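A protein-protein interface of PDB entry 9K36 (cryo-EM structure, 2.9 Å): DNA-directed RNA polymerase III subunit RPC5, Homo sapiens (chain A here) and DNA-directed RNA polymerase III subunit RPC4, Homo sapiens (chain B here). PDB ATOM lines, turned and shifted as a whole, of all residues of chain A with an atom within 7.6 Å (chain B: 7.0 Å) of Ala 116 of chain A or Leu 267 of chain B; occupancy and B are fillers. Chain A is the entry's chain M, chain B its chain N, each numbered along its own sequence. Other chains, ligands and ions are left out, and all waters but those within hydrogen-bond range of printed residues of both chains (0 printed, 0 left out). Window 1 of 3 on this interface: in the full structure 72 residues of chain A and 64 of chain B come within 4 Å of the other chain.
Hydrophobic or aromatic side chains of chain B within 4 Å of the printed part of chain A: Leu 266, Leu 267, Phe 268, Leu 269, Leu 318, Leu 360 and Leu 376. Printed residues of chain A that touch a printed residue of chain B: Leu 25, Tyr 26, Leu 27, Tyr 114, Ala 115, Ala 116, Ala 117, Leu 118, Tyr 119, Leu 124, Leu 126, Pro 128, Leu 129 and Leu 225. Hydrophobic or aromatic side chains of chain A that line the printed part of chain B: Leu 25, Leu 27, Tyr 114, Ala 115, Ala 116, Ala 117, Leu 118, Tyr 119, Leu 124, Leu 126, Pro 128, Leu 129 and Leu 225. Among the printed residues, no Asp or Glu carboxylate lies within 4 Å of a Lys or Arg side-chain nitrogen of the other chain.
Leu 25 of chain A touches Leu 360 of chain B. Leu 25 of chain A touches Leu 376 of chain B. Phe 268 of chain B touches Ala 115 of chain A. Ala 116 of chain A touches Leu 360 of chain B. O of Ala 117 of chain A touches O of Glu 265 of chain B (3.9 Å). Ala 117 of chain A touches Leu 266 of chain B (O to C, 3.4 Å). Leu 269 of chain B touches Ala 117 of chain A (CD2 to CB, 3.7 Å). CB of Leu 118 of chain A touches CD1 of Leu 266 of chain B, at 3.7 Å. CD2 of Leu 269 of chain B touches CD2 of Leu 126 of chain A, 3.7 Å away. Leu 318 of chain B touches Pro 128 of chain A (CB to CG, 3.7 Å).
Tyr 16 of chain A touches none of the printed residues of chain B. Of the printed residues of chain B, Ala 115 of chain A touches Phe 268 (3.5 Å), Leu 269 (3.2 Å) and Leu 318 (3.7 Å). Of chain B, only Leu 267 (3.6 Å) and Leu 360 (3.7 Å) come within 4 Å of Ala 116 of chain A. Printed residues of chain B within 4 Å of Ala 117 of chain A: Glu 265, Leu 266, Leu 267 and Leu 269. Printed residues of chain B within 4 Å of Leu 118 of chain A: Glu 265 (3.9 Å) and Leu 266 (3.7 Å). Printed residues of chain B within 4 Å of Pro 128 of chain A: Leu 318. Leu 267 of chain B touches just these residues of chain A: Ala 116 and Ala 117. The nearest printed residue of chain A that does not touch Leu 269 of chain B is Tyr 114 of chain A (4.4 Å).
The backbone carbonyl oxygen (O) of Leu 124 of chain A lies within hydrogen-bond range of the backbone NH (N) of Tyr 16 of chain A (2.9 Å). The backbone carbonyl oxygen of Tyr 16 of chain A is in hydrogen-bond range of the backbone NH of Leu 126 of chain A (2.9 Å). The backbone NH (N) of Ala 116 of chain A lies within hydrogen-bond range of the backbone carbonyl oxygen (O) of Thr 127 of chain A, 2.9 Å away. N of His 125 of chain A is in hydrogen-bond range of O of Leu 118 of chain A (2.9 Å). The backbone carbonyl oxygen (O) of Phe 268 of chain B sits at hydrogen-bond distance from the backbone NH (N) of Leu 383 of chain B, at 3.0 Å. O of Leu 360 of chain B lies within hydrogen-bond range of N of Leu 376 of chain B (2.9 Å).
The backbone NH (N) of Leu 269 of chain B sits at hydrogen-bond distance from the backbone carbonyl oxygen (O) of Ala 115 of chain A (3.4 Å). N of Leu 267 of chain B lies within hydrogen-bond range of O of Ala 117 of chain A (2.5 Å). The backbone NH (N) of Tyr 119 of chain A is in hydrogen-bond range of the backbone carbonyl oxygen (O) of Glu 265 of chain B (2.9 Å).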
ATOM      1  N   TYR A  16      11.563  -5.967 -23.844  1.00  0.00           N
ATOM      2  CA  TYR A  16      11.386  -7.020 -22.858  1.00  0.00           C
ATOM      3  C   TYR A  16      11.302  -6.420 -21.460  1.00  0.00           C
ATOM      4  O   TYR A  16      11.729  -5.290 -21.218  1.00  0.00           O
ATOM      5  CB  TYR A  16      12.532  -8.034 -22.925  1.00  0.00           C
ATOM      6  CG  TYR A  16      12.687  -8.712 -24.269  1.00  0.00           C
ATOM      7  CD1 TYR A  16      11.592  -8.909 -25.102  1.00  0.00           C
ATOM      8  CD2 TYR A  16      13.927  -9.157 -24.706  1.00  0.00           C
ATOM      9  CE1 TYR A  16      11.729  -9.528 -26.329  1.00  0.00           C
ATOM     10  CE2 TYR A  16      14.076  -9.778 -25.930  1.00  0.00           C
ATOM     11  CZ  TYR A  16      12.973  -9.960 -26.739  1.00  0.00           C
ATOM     12  OH  TYR A  16      13.114 -10.578 -27.960  1.00  0.00           O
ATOM     13  N   LEU A  25      16.882  -2.330  -7.381  1.00  0.00           N
ATOM     14  CA  LEU A  25      17.491  -1.398  -8.320  1.00  0.00           C
ATOM     15  C   LEU A  25      17.323   0.027  -7.808  1.00  0.00           C
ATOM     16  O   LEU A  25      16.195   0.497  -7.626  1.00  0.00           O
ATOM     17  CB  LEU A  25      16.868  -1.544  -9.710  1.00  0.00           C
ATOM     18  CG  LEU A  25      17.536  -0.764 -10.843  1.00  0.00           C
ATOM     19  CD1 LEU A  25      18.987  -1.186 -10.990  1.00  0.00           C
ATOM     20  CD2 LEU A  25      16.782  -0.966 -12.148  1.00  0.00           C
ATOM     21  N   TYR A  26      18.444   0.709  -7.583  1.00  0.00           N
ATOM     22  CA  TYR A  26      18.455   2.102  -7.166  1.00  0.00           C
ATOM     23  C   TYR A  26      19.219   2.939  -8.181  1.00  0.00           C
ATOM     24  O   TYR A  26      20.122   2.447  -8.865  1.00  0.00           O
ATOM     25  CB  TYR A  26      19.088   2.269  -5.777  1.00  0.00           C
ATOM     26  CG  TYR A  26      18.204   1.817  -4.635  1.00  0.00           C
ATOM     27  CD1 TYR A  26      16.825   1.745  -4.784  1.00  0.00           C
ATOM     28  CD2 TYR A  26      18.750   1.466  -3.407  1.00  0.00           C
ATOM     29  CE1 TYR A  26      16.015   1.335  -3.742  1.00  0.00           C
ATOM     30  CE2 TYR A  26      17.949   1.054  -2.361  1.00  0.00           C
ATOM     31  CZ  TYR A  26      16.582   0.989  -2.534  1.00  0.00           C
ATOM     32  OH  TYR A  26      15.780   0.580  -1.492  1.00  0.00           O
ATOM     33  N   LEU A  27      18.853   4.214  -8.273  1.00  0.00           N
ATOM     34  CA  LEU A  27      19.492   5.158  -9.180  1.00  0.00           C
ATOM     35  C   LEU A  27      20.192   6.233  -8.360  1.00  0.00           C
ATOM     36  O   LEU A  27      19.537   6.994  -7.639  1.00  0.00           O
ATOM     37  CB  LEU A  27      18.469   5.785 -10.129  1.00  0.00           C
ATOM     38  CG  LEU A  27      19.015   6.764 -11.170  1.00  0.00           C
ATOM     39  CD1 LEU A  27      20.051   6.086 -12.053  1.00  0.00           C
ATOM     40  CD2 LEU A  27      17.884   7.336 -12.010  1.00  0.00           C
ATOM     41  N   TYR A 114       9.241   5.351 -13.443  1.00  0.00           N
ATOM     42  CA  TYR A 114      10.621   5.394 -13.904  1.00  0.00           C
ATOM     43  C   TYR A 114      11.154   3.977 -14.067  1.00  0.00           C
ATOM     44  O   TYR A 114      10.834   3.088 -13.272  1.00  0.00           O
ATOM     45  CB  TYR A 114      11.499   6.180 -12.929  1.00  0.00           C
ATOM     46  CG  TYR A 114      11.008   7.583 -12.659  1.00  0.00           C
ATOM     47  CD1 TYR A 114      11.311   8.625 -13.527  1.00  0.00           C
ATOM     48  CD2 TYR A 114      10.242   7.868 -11.535  1.00  0.00           C
ATOM     49  CE1 TYR A 114      10.863   9.911 -13.282  1.00  0.00           C
ATOM     50  CE2 TYR A 114       9.791   9.149 -11.283  1.00  0.00           C
ATOM     51  CZ  TYR A 114      10.103  10.167 -12.159  1.00  0.00           C
ATOM     52  OH  TYR A 114       9.655  11.443 -11.911  1.00  0.00           O
ATOM     53  N   ALA A 115      11.970   3.772 -15.098  1.00  0.00           N
ATOM     54  CA  ALA A 115      12.506   2.455 -15.405  1.00  0.00           C
ATOM     55  C   ALA A 115      13.879   2.590 -16.044  1.00  0.00           C
ATOM     56  O   ALA A 115      14.144   3.549 -16.773  1.00  0.00           O
ATOM     57  CB  ALA A 115      11.569   1.674 -16.334  1.00  0.00           C
ATOM     58  N   ALA A 116      14.746   1.621 -15.762  1.00  0.00           N
ATOM     59  CA  ALA A 116      16.069   1.555 -16.365  1.00  0.00           C
ATOM     60  C   ALA A 116      16.010   0.682 -17.608  1.00  0.00           C
ATOM     61  O   ALA A 116      15.413  -0.400 -17.587  1.00  0.00           O
ATOM     62  CB  ALA A 116      17.093   1.003 -15.370  1.00  0.00           C
ATOM     63  N   ALA A 117      16.629   1.151 -18.689  1.00  0.00           N
ATOM     64  CA  ALA A 117      16.573   0.493 -19.988  1.00  0.00           C
ATOM     65  C   ALA A 117      17.975   0.047 -20.384  1.00  0.00           C
ATOM     66  O   ALA A 117      18.855   0.883 -20.616  1.00  0.00           O
ATOM     67  CB  ALA A 117      15.976   1.426 -21.039  1.00  0.00           C
ATOM     68  N   LEU A 118      18.176  -1.265 -20.458  1.00  0.00           N
ATOM     69  CA  LEU A 118      19.423  -1.835 -20.954  1.00  0.00           C
ATOM     70  C   LEU A 118      19.238  -2.236 -22.413  1.00  0.00           C
ATOM     71  O   LEU A 118      18.342  -3.024 -22.735  1.00  0.00           O
ATOM     72  CB  LEU A 118      19.847  -3.035 -20.107  1.00  0.00           C
ATOM     73  CG  LEU A 118      21.253  -3.603 -20.326  1.00  0.00           C
ATOM     74  CD1 LEU A 118      21.830  -4.119 -19.020  1.00  0.00           C
ATOM     75  CD2 LEU A 118      21.239  -4.712 -21.365  1.00  0.00           C
ATOM     76  N   TYR A 119      20.083  -1.700 -23.288  1.00  0.00           N
ATOM     77  CA  TYR A 119      19.946  -1.883 -24.726  1.00  0.00           C
ATOM     78  C   TYR A 119      20.960  -2.903 -25.223  1.00  0.00           C
ATOM     79  O   TYR A 119      22.167  -2.735 -25.017  1.00  0.00           O
ATOM     80  CB  TYR A 119      20.127  -0.552 -25.459  1.00  0.00           C
ATOM     81  CG  TYR A 119      20.045  -0.657 -26.965  1.00  0.00           C
ATOM     82  CD1 TYR A 119      18.818  -0.727 -27.609  1.00  0.00           C
ATOM     83  CD2 TYR A 119      21.196  -0.676 -27.745  1.00  0.00           C
ATOM     84  CE1 TYR A 119      18.737  -0.821 -28.987  1.00  0.00           C
ATOM     85  CE2 TYR A 119      21.126  -0.769 -29.122  1.00  0.00           C
ATOM     86  CZ  TYR A 119      19.893  -0.841 -29.737  1.00  0.00           C
ATOM     87  OH  TYR A 119      19.817  -0.934 -31.108  1.00  0.00           O
ATOM     88  N   LEU A 124      15.524  -4.191 -26.021  1.00  0.00           N
ATOM     89  CA  LEU A 124      15.614  -3.218 -24.938  1.00  0.00           C
ATOM     90  C   LEU A 124      14.896  -3.785 -23.724  1.00  0.00           C
ATOM     91  O   LEU A 124      13.684  -4.016 -23.772  1.00  0.00           O
ATOM     92  CB  LEU A 124      15.003  -1.875 -25.348  1.00  0.00           C
ATOM     93  CG  LEU A 124      15.152  -0.729 -24.349  1.00  0.00           C
ATOM     94  CD1 LEU A 124      16.617  -0.383 -24.155  1.00  0.00           C
ATOM     95  CD2 LEU A 124      14.364   0.492 -24.805  1.00  0.00           C
ATOM     96  N   HIS A 125      15.638  -4.019 -22.646  1.00  0.00           N
ATOM     97  CA  HIS A 125      15.093  -4.600 -21.426  1.00  0.00           C
ATOM     98  C   HIS A 125      14.799  -3.497 -20.418  1.00  0.00           C
ATOM     99  O   HIS A 125      15.672  -2.677 -20.116  1.00  0.00           O
ATOM    100  CB  HIS A 125      16.066  -5.616 -20.824  1.00  0.00           C
ATOM    101  CG  HIS A 125      16.359  -6.780 -21.721  1.00  0.00           C
ATOM    102  ND1 HIS A 125      15.946  -8.062 -21.431  1.00  0.00           N
ATOM    103  CD2 HIS A 125      17.022  -6.853 -22.898  1.00  0.00           C
ATOM    104  CE1 HIS A 125      16.344  -8.875 -22.392  1.00  0.00           C
ATOM    105  NE2 HIS A 125      16.998  -8.168 -23.296  1.00  0.00           N
ATOM    106  N   LEU A 126      13.576  -3.484 -19.899  1.00  0.00           N
ATOM    107  CA  LEU A 126      13.150  -2.496 -18.920  1.00  0.00           C
ATOM    108  C   LEU A 126      13.096  -3.123 -17.532  1.00  0.00           C
ATOM    109  O   LEU A 126      12.665  -4.268 -17.373  1.00  0.00           O
ATOM    110  CB  LEU A 126      11.780  -1.922 -19.284  1.00  0.00           C
ATOM    111  CG  LEU A 126      11.631  -1.352 -20.696  1.00  0.00           C
ATOM    112  CD1 LEU A 126      10.260  -0.723 -20.878  1.00  0.00           C
ATOM    113  CD2 LEU A 126      12.732  -0.348 -20.989  1.00  0.00           C
ATOM    114  N   THR A 127      13.539  -2.363 -16.528  1.00  0.00           N
ATOM    115  CA  THR A 127      13.526  -2.827 -15.148  1.00  0.00           C
ATOM    116  C   THR A 127      13.017  -1.699 -14.257  1.00  0.00           C
ATOM    117  O   THR A 127      13.555  -0.578 -14.314  1.00  0.00           O
ATOM    118  CB  THR A 127      14.913  -3.286 -14.691  1.00  0.00           C
ATOM    119  OG1 THR A 127      15.415  -4.276 -15.595  1.00  0.00           O
ATOM    120  CG2 THR A 127      14.843  -3.879 -13.292  1.00  0.00           C
ATOM    121  N   PRO A 128      11.995  -1.948 -13.440  1.00  0.00           N
ATOM    122  CA  PRO A 128      11.475  -0.891 -12.567  1.00  0.00           C
ATOM    123  C   PRO A 128      12.492  -0.469 -11.518  1.00  0.00           C
ATOM    124  O   PRO A 128      13.376  -1.238 -11.127  1.00  0.00           O
ATOM    125  CB  PRO A 128      10.247  -1.538 -11.915  1.00  0.00           C
ATOM    126  CG  PRO A 128       9.886  -2.678 -12.814  1.00  0.00           C
ATOM    127  CD  PRO A 128      11.186  -3.175 -13.368  1.00  0.00           C
ATOM    128  N   LEU A 129      12.354   0.773 -11.061  1.00  0.00           N
ATOM    129  CA  LEU A 129      13.230   1.347 -10.051  1.00  0.00           C
ATOM    130  C   LEU A 129      12.518   1.383  -8.706  1.00  0.00           C
ATOM    131  O   LEU A 129      11.396   1.893  -8.607  1.00  0.00           O
ATOM    132  CB  LEU A 129      13.676   2.758 -10.446  1.00  0.00           C
ATOM    133  CG  LEU A 129      14.984   2.894 -11.230  1.00  0.00           C
ATOM    134  CD1 LEU A 129      14.909   2.150 -12.548  1.00  0.00           C
ATOM    135  CD2 LEU A 129      15.322   4.357 -11.461  1.00  0.00           C
ATOM    136  N   LEU A 225      19.447  -8.001 -15.315  1.00  0.00           N
ATOM    137  CA  LEU A 225      18.531  -7.067 -15.959  1.00  0.00           C
ATOM    138  C   LEU A 225      17.854  -7.662 -17.185  1.00  0.00           C
ATOM    139  O   LEU A 225      16.894  -7.068 -17.688  1.00  0.00           O
ATOM    140  CB  LEU A 225      19.271  -5.784 -16.345  1.00  0.00           C
ATOM    141  CG  LEU A 225      19.765  -4.916 -15.188  1.00  0.00           C
ATOM    142  CD1 LEU A 225      20.359  -3.615 -15.710  1.00  0.00           C
ATOM    143  CD2 LEU A 225      18.641  -4.638 -14.205  1.00  0.00           C
ATOM    144  N   GLU B 253      20.147   8.588 -32.636  1.00  0.00           N
ATOM    145  CA  GLU B 253      20.771   8.004 -31.453  1.00  0.00           C
ATOM    146  C   GLU B 253      20.802   6.483 -31.544  1.00  0.00           C
ATOM    147  O   GLU B 253      21.863   5.860 -31.434  1.00  0.00           O
ATOM    148  CB  GLU B 253      20.025   8.457 -30.196  1.00  0.00           C
ATOM    149  CG  GLU B 253      20.586   7.893 -28.896  1.00  0.00           C
ATOM    150  CD  GLU B 253      21.927   8.496 -28.523  1.00  0.00           C
ATOM    151  OE1 GLU B 253      22.275   9.567 -29.066  1.00  0.00           O
ATOM    152  OE2 GLU B 253      22.636   7.898 -27.687  1.00  0.00           O
ATOM    153  N   LEU B 254      19.637   5.867 -31.761  1.00  0.00           N
ATOM    154  CA  LEU B 254      19.581   4.412 -31.876  1.00  0.00           C
ATOM    155  C   LEU B 254      20.340   3.922 -33.105  1.00  0.00           C
ATOM    156  O   LEU B 254      20.960   2.850 -33.073  1.00  0.00           O
ATOM    157  CB  LEU B 254      18.128   3.943 -31.915  1.00  0.00           C
ATOM    158  CG  LEU B 254      17.285   4.260 -30.678  1.00  0.00           C
ATOM    159  CD1 LEU B 254      15.874   3.713 -30.831  1.00  0.00           C
ATOM    160  CD2 LEU B 254      17.945   3.708 -29.426  1.00  0.00           C
ATOM    161  N   GLU B 257      23.848   3.891 -32.215  1.00  0.00           N
ATOM    162  CA  GLU B 257      24.066   2.903 -31.165  1.00  0.00           C
ATOM    163  C   GLU B 257      24.086   1.481 -31.712  1.00  0.00           C
ATOM    164  O   GLU B 257      24.720   0.603 -31.118  1.00  0.00           O
ATOM    165  CB  GLU B 257      22.995   3.034 -30.081  1.00  0.00           C
ATOM    166  CG  GLU B 257      23.220   4.183 -29.110  1.00  0.00           C
ATOM    167  CD  GLU B 257      22.146   4.261 -28.043  1.00  0.00           C
ATOM    168  OE1 GLU B 257      21.163   3.498 -28.131  1.00  0.00           O
ATOM    169  OE2 GLU B 257      22.288   5.082 -27.114  1.00  0.00           O
ATOM    170  N   GLU B 265      24.398  -0.164 -24.252  1.00  0.00           N
ATOM    171  CA  GLU B 265      24.226   1.132 -23.617  1.00  0.00           C
ATOM    172  C   GLU B 265      23.074   1.064 -22.625  1.00  0.00           C
ATOM    173  O   GLU B 265      22.063   0.399 -22.869  1.00  0.00           O
ATOM    174  CB  GLU B 265      23.968   2.233 -24.658  1.00  0.00           C
ATOM    175  CG  GLU B 265      23.806   3.630 -24.077  1.00  0.00           C
ATOM    176  CD  GLU B 265      25.082   4.160 -23.456  1.00  0.00           C
ATOM    177  OE1 GLU B 265      26.174   3.694 -23.842  1.00  0.00           O
ATOM    178  OE2 GLU B 265      24.992   5.045 -22.580  1.00  0.00           O
ATOM    179  N   LEU B 266      23.239   1.755 -21.502  1.00  0.00           N
ATOM    180  CA  LEU B 266      22.223   1.828 -20.459  1.00  0.00           C
ATOM    181  C   LEU B 266      21.425   3.114 -20.634  1.00  0.00           C
ATOM    182  O   LEU B 266      21.997   4.209 -20.633  1.00  0.00           O
ATOM    183  CB  LEU B 266      22.854   1.770 -19.070  1.00  0.00           C
ATOM    184  CG  LEU B 266      23.086   0.392 -18.447  1.00  0.00           C
ATOM    185  CD1 LEU B 266      21.774  -0.371 -18.336  1.00  0.00           C
ATOM    186  CD2 LEU B 266      24.114  -0.410 -19.230  1.00  0.00           C
ATOM    187  N   LEU B 267      20.110   2.982 -20.782  1.00  0.00           N
ATOM    188  CA  LEU B 267      19.218   4.114 -20.966  1.00  0.00           C
ATOM    189  C   LEU B 267      18.268   4.236 -19.781  1.00  0.00           C
ATOM    190  O   LEU B 267      18.043   3.281 -19.033  1.00  0.00           O
ATOM    191  CB  LEU B 267      18.418   3.977 -22.266  1.00  0.00           C
ATOM    192  CG  LEU B 267      19.231   3.902 -23.560  1.00  0.00           C
ATOM    193  CD1 LEU B 267      18.309   3.762 -24.763  1.00  0.00           C
ATOM    194  CD2 LEU B 267      20.121   5.126 -23.702  1.00  0.00           C
ATOM    195  N   PHE B 268      17.712   5.435 -19.622  1.00  0.00           N
ATOM    196  CA  PHE B 268      16.756   5.732 -18.555  1.00  0.00           C
ATOM    197  C   PHE B 268      15.555   6.428 -19.190  1.00  0.00           C
ATOM    198  O   PHE B 268      15.593   7.635 -19.450  1.00  0.00           O
ATOM    199  CB  PHE B 268      17.395   6.595 -17.471  1.00  0.00           C
ATOM    200  CG  PHE B 268      16.443   7.015 -16.387  1.00  0.00           C
ATOM    201  CD1 PHE B 268      16.080   6.133 -15.382  1.00  0.00           C
ATOM    202  CD2 PHE B 268      15.916   8.297 -16.367  1.00  0.00           C
ATOM    203  CE1 PHE B 268      15.206   6.517 -14.384  1.00  0.00           C
ATOM    204  CE2 PHE B 268      15.042   8.688 -15.370  1.00  0.00           C
ATOM    205  CZ  PHE B 268      14.688   7.796 -14.378  1.00  0.00           C
ATOM    206  N   LEU B 269      14.493   5.670 -19.441  1.00  0.00           N
ATOM    207  CA  LEU B 269      13.288   6.191 -20.068  1.00  0.00           C
ATOM    208  C   LEU B 269      12.192   6.376 -19.027  1.00  0.00           C
ATOM    209  O   LEU B 269      12.081   5.591 -18.080  1.00  0.00           O
ATOM    210  CB  LEU B 269      12.808   5.269 -21.195  1.00  0.00           C
ATOM    211  CG  LEU B 269      12.863   3.747 -21.018  1.00  0.00           C
ATOM    212  CD1 LEU B 269      11.690   3.226 -20.200  1.00  0.00           C
ATOM    213  CD2 LEU B 269      12.911   3.072 -22.377  1.00  0.00           C
ATOM    214  N   LEU B 318       4.870  -1.159 -14.461  1.00  0.00           N
ATOM    215  CA  LEU B 318       5.690  -2.314 -14.805  1.00  0.00           C
ATOM    216  C   LEU B 318       5.734  -3.349 -13.688  1.00  0.00           C
ATOM    217  O   LEU B 318       6.051  -4.512 -13.952  1.00  0.00           O
ATOM    218  CB  LEU B 318       7.111  -1.871 -15.149  1.00  0.00           C
ATOM    219  CG  LEU B 318       7.276  -0.924 -16.340  1.00  0.00           C
ATOM    220  CD1 LEU B 318       8.751  -0.651 -16.593  1.00  0.00           C
ATOM    221  CD2 LEU B 318       6.613  -1.496 -17.580  1.00  0.00           C
ATOM    222  N   LEU B 360      23.892   3.810 -12.487  1.00  0.00           N
ATOM    223  CA  LEU B 360      22.846   2.828 -12.230  1.00  0.00           C
ATOM    224  C   LEU B 360      23.460   1.641 -11.499  1.00  0.00           C
ATOM    225  O   LEU B 360      24.306   0.930 -12.056  1.00  0.00           O
ATOM    226  CB  LEU B 360      22.199   2.383 -13.540  1.00  0.00           C
ATOM    227  CG  LEU B 360      21.082   1.343 -13.436  1.00  0.00           C
ATOM    228  CD1 LEU B 360      19.859   1.935 -12.757  1.00  0.00           C
ATOM    229  CD2 LEU B 360      20.731   0.793 -14.810  1.00  0.00           C
ATOM    230  N   LEU B 376      25.877  -1.432 -11.776  1.00  0.00           N
ATOM    231  CA  LEU B 376      25.537  -2.048 -13.053  1.00  0.00           C
ATOM    232  C   LEU B 376      26.147  -1.285 -14.222  1.00  0.00           C
ATOM    233  O   LEU B 376      26.642  -1.897 -15.177  1.00  0.00           O
ATOM    234  CB  LEU B 376      24.018  -2.140 -13.200  1.00  0.00           C
ATOM    235  CG  LEU B 376      23.307  -2.996 -12.150  1.00  0.00           C
ATOM    236  CD1 LEU B 376      21.808  -3.015 -12.396  1.00  0.00           C
ATOM    237  CD2 LEU B 376      23.865  -4.410 -12.139  1.00  0.00           C
ATOM    238  N   HIS B 378      26.680   3.067 -16.106  1.00  0.00           N
ATOM    239  CA  HIS B 378      26.514   4.513 -16.091  1.00  0.00           C
ATOM    240  C   HIS B 378      25.351   4.912 -16.992  1.00  0.00           C
ATOM    241  O   HIS B 378      25.120   4.293 -18.036  1.00  0.00           O
ATOM    242  CB  HIS B 378      27.794   5.217 -16.548  1.00  0.00           C
ATOM    243  CG  HIS B 378      28.977   4.941 -15.672  1.00  0.00           C
ATOM    244  ND1 HIS B 378      29.234   5.658 -14.523  1.00  0.00           N
ATOM    245  CD2 HIS B 378      29.971   4.026 -15.776  1.00  0.00           C
ATOM    246  CE1 HIS B 378      30.336   5.197 -13.957  1.00  0.00           C
ATOM    247  NE2 HIS B 378      30.803   4.208 -14.697  1.00  0.00           N
ATOM    248  N   VAL B 379      24.626   5.949 -16.581  1.00  0.00           N
ATOM    249  CA  VAL B 379      23.492   6.474 -17.333  1.00  0.00           C
ATOM    250  C   VAL B 379      23.914   7.776 -17.994  1.00  0.00           C
ATOM    251  O   VAL B 379      24.419   8.688 -17.324  1.00  0.00           O
ATOM    252  CB  VAL B 379      22.270   6.688 -16.424  1.00  0.00           C
ATOM    253  CG1 VAL B 379      21.095   7.224 -17.228  1.00  0.00           C
ATOM    254  CG2 VAL B 379      21.899   5.389 -15.723  1.00  0.00           C
ATOM    255  N   LYS B 380      23.706   7.869 -19.307  1.00  0.00           N
ATOM    256  CA  LYS B 380      24.106   9.037 -20.082  1.00  0.00           C
ATOM    257  C   LYS B 380      22.927   9.754 -20.727  1.00  0.00           C
ATOM    258  O   LYS B 380      22.830  10.982 -20.642  1.00  0.00           O
ATOM    259  CB  LYS B 380      25.118   8.627 -21.162  1.00  0.00           C
ATOM    260  CG  LYS B 380      25.638   9.784 -21.997  1.00  0.00           C
ATOM    261  CD  LYS B 380      26.415  10.772 -21.149  1.00  0.00           C
ATOM    262  CE  LYS B 380      27.657  10.131 -20.551  1.00  0.00           C
ATOM    263  NZ  LYS B 380      28.585   9.639 -21.604  1.00  0.00           N
ATOM    264  N   HIS B 381      22.026   9.016 -21.370  1.00  0.00           N
ATOM    265  CA  HIS B 381      20.896   9.601 -22.075  1.00  0.00           C
ATOM    266  C   HIS B 381      19.598   9.276 -21.352  1.00  0.00           C
ATOM    267  O   HIS B 381      19.485   8.252 -20.672  1.00  0.00           O
ATOM    268  CB  HIS B 381      20.821   9.095 -23.521  1.00  0.00           C
ATOM    269  CG  HIS B 381      22.075   9.324 -24.307  1.00  0.00           C
ATOM    270  ND1 HIS B 381      23.174   8.498 -24.208  1.00  0.00           N
ATOM    271  CD2 HIS B 381      22.407  10.285 -25.199  1.00  0.00           C
ATOM    272  CE1 HIS B 381      24.128   8.940 -25.008  1.00  0.00           C
ATOM    273  NE2 HIS B 381      23.688  10.026 -25.620  1.00  0.00           N
ATOM    274  N   LYS B 382      18.617  10.164 -21.504  1.00  0.00           N
ATOM    275  CA  LYS B 382      17.304  10.008 -20.896  1.00  0.00           C
ATOM    276  C   LYS B 382      16.234  10.108 -21.972  1.00  0.00           C
ATOM    277  O   LYS B 382      16.269  11.021 -22.806  1.00  0.00           O
ATOM    278  CB  LYS B 382      17.068  11.066 -19.813  1.00  0.00           C
ATOM    279  CG  LYS B 382      15.713  10.959 -19.129  1.00  0.00           C
ATOM    280  CD  LYS B 382      15.535  12.047 -18.082  1.00  0.00           C
ATOM    281  CE  LYS B 382      14.170  11.953 -17.417  1.00  0.00           C
ATOM    282  NZ  LYS B 382      13.967  13.028 -16.405  1.00  0.00           N
ATOM    283  N   LEU B 383      15.290   9.173 -21.954  1.00  0.00           N
ATOM    284  CA  LEU B 383      14.185   9.139 -22.898  1.00  0.00           C
ATOM    285  C   LEU B 383      12.876   9.441 -22.181  1.00  0.00           C
ATOM    286  O   LEU B 383      12.748   9.229 -20.972  1.00  0.00           O
ATOM    287  CB  LEU B 383      14.096   7.776 -23.593  1.00  0.00           C
ATOM    288  CG  LEU B 383      15.340   7.312 -24.354  1.00  0.00           C
ATOM    289  CD1 LEU B 383      15.113   5.937 -24.966  1.00  0.00           C
ATOM    290  CD2 LEU B 383      15.724   8.318 -25.427  1.00  0.00           C
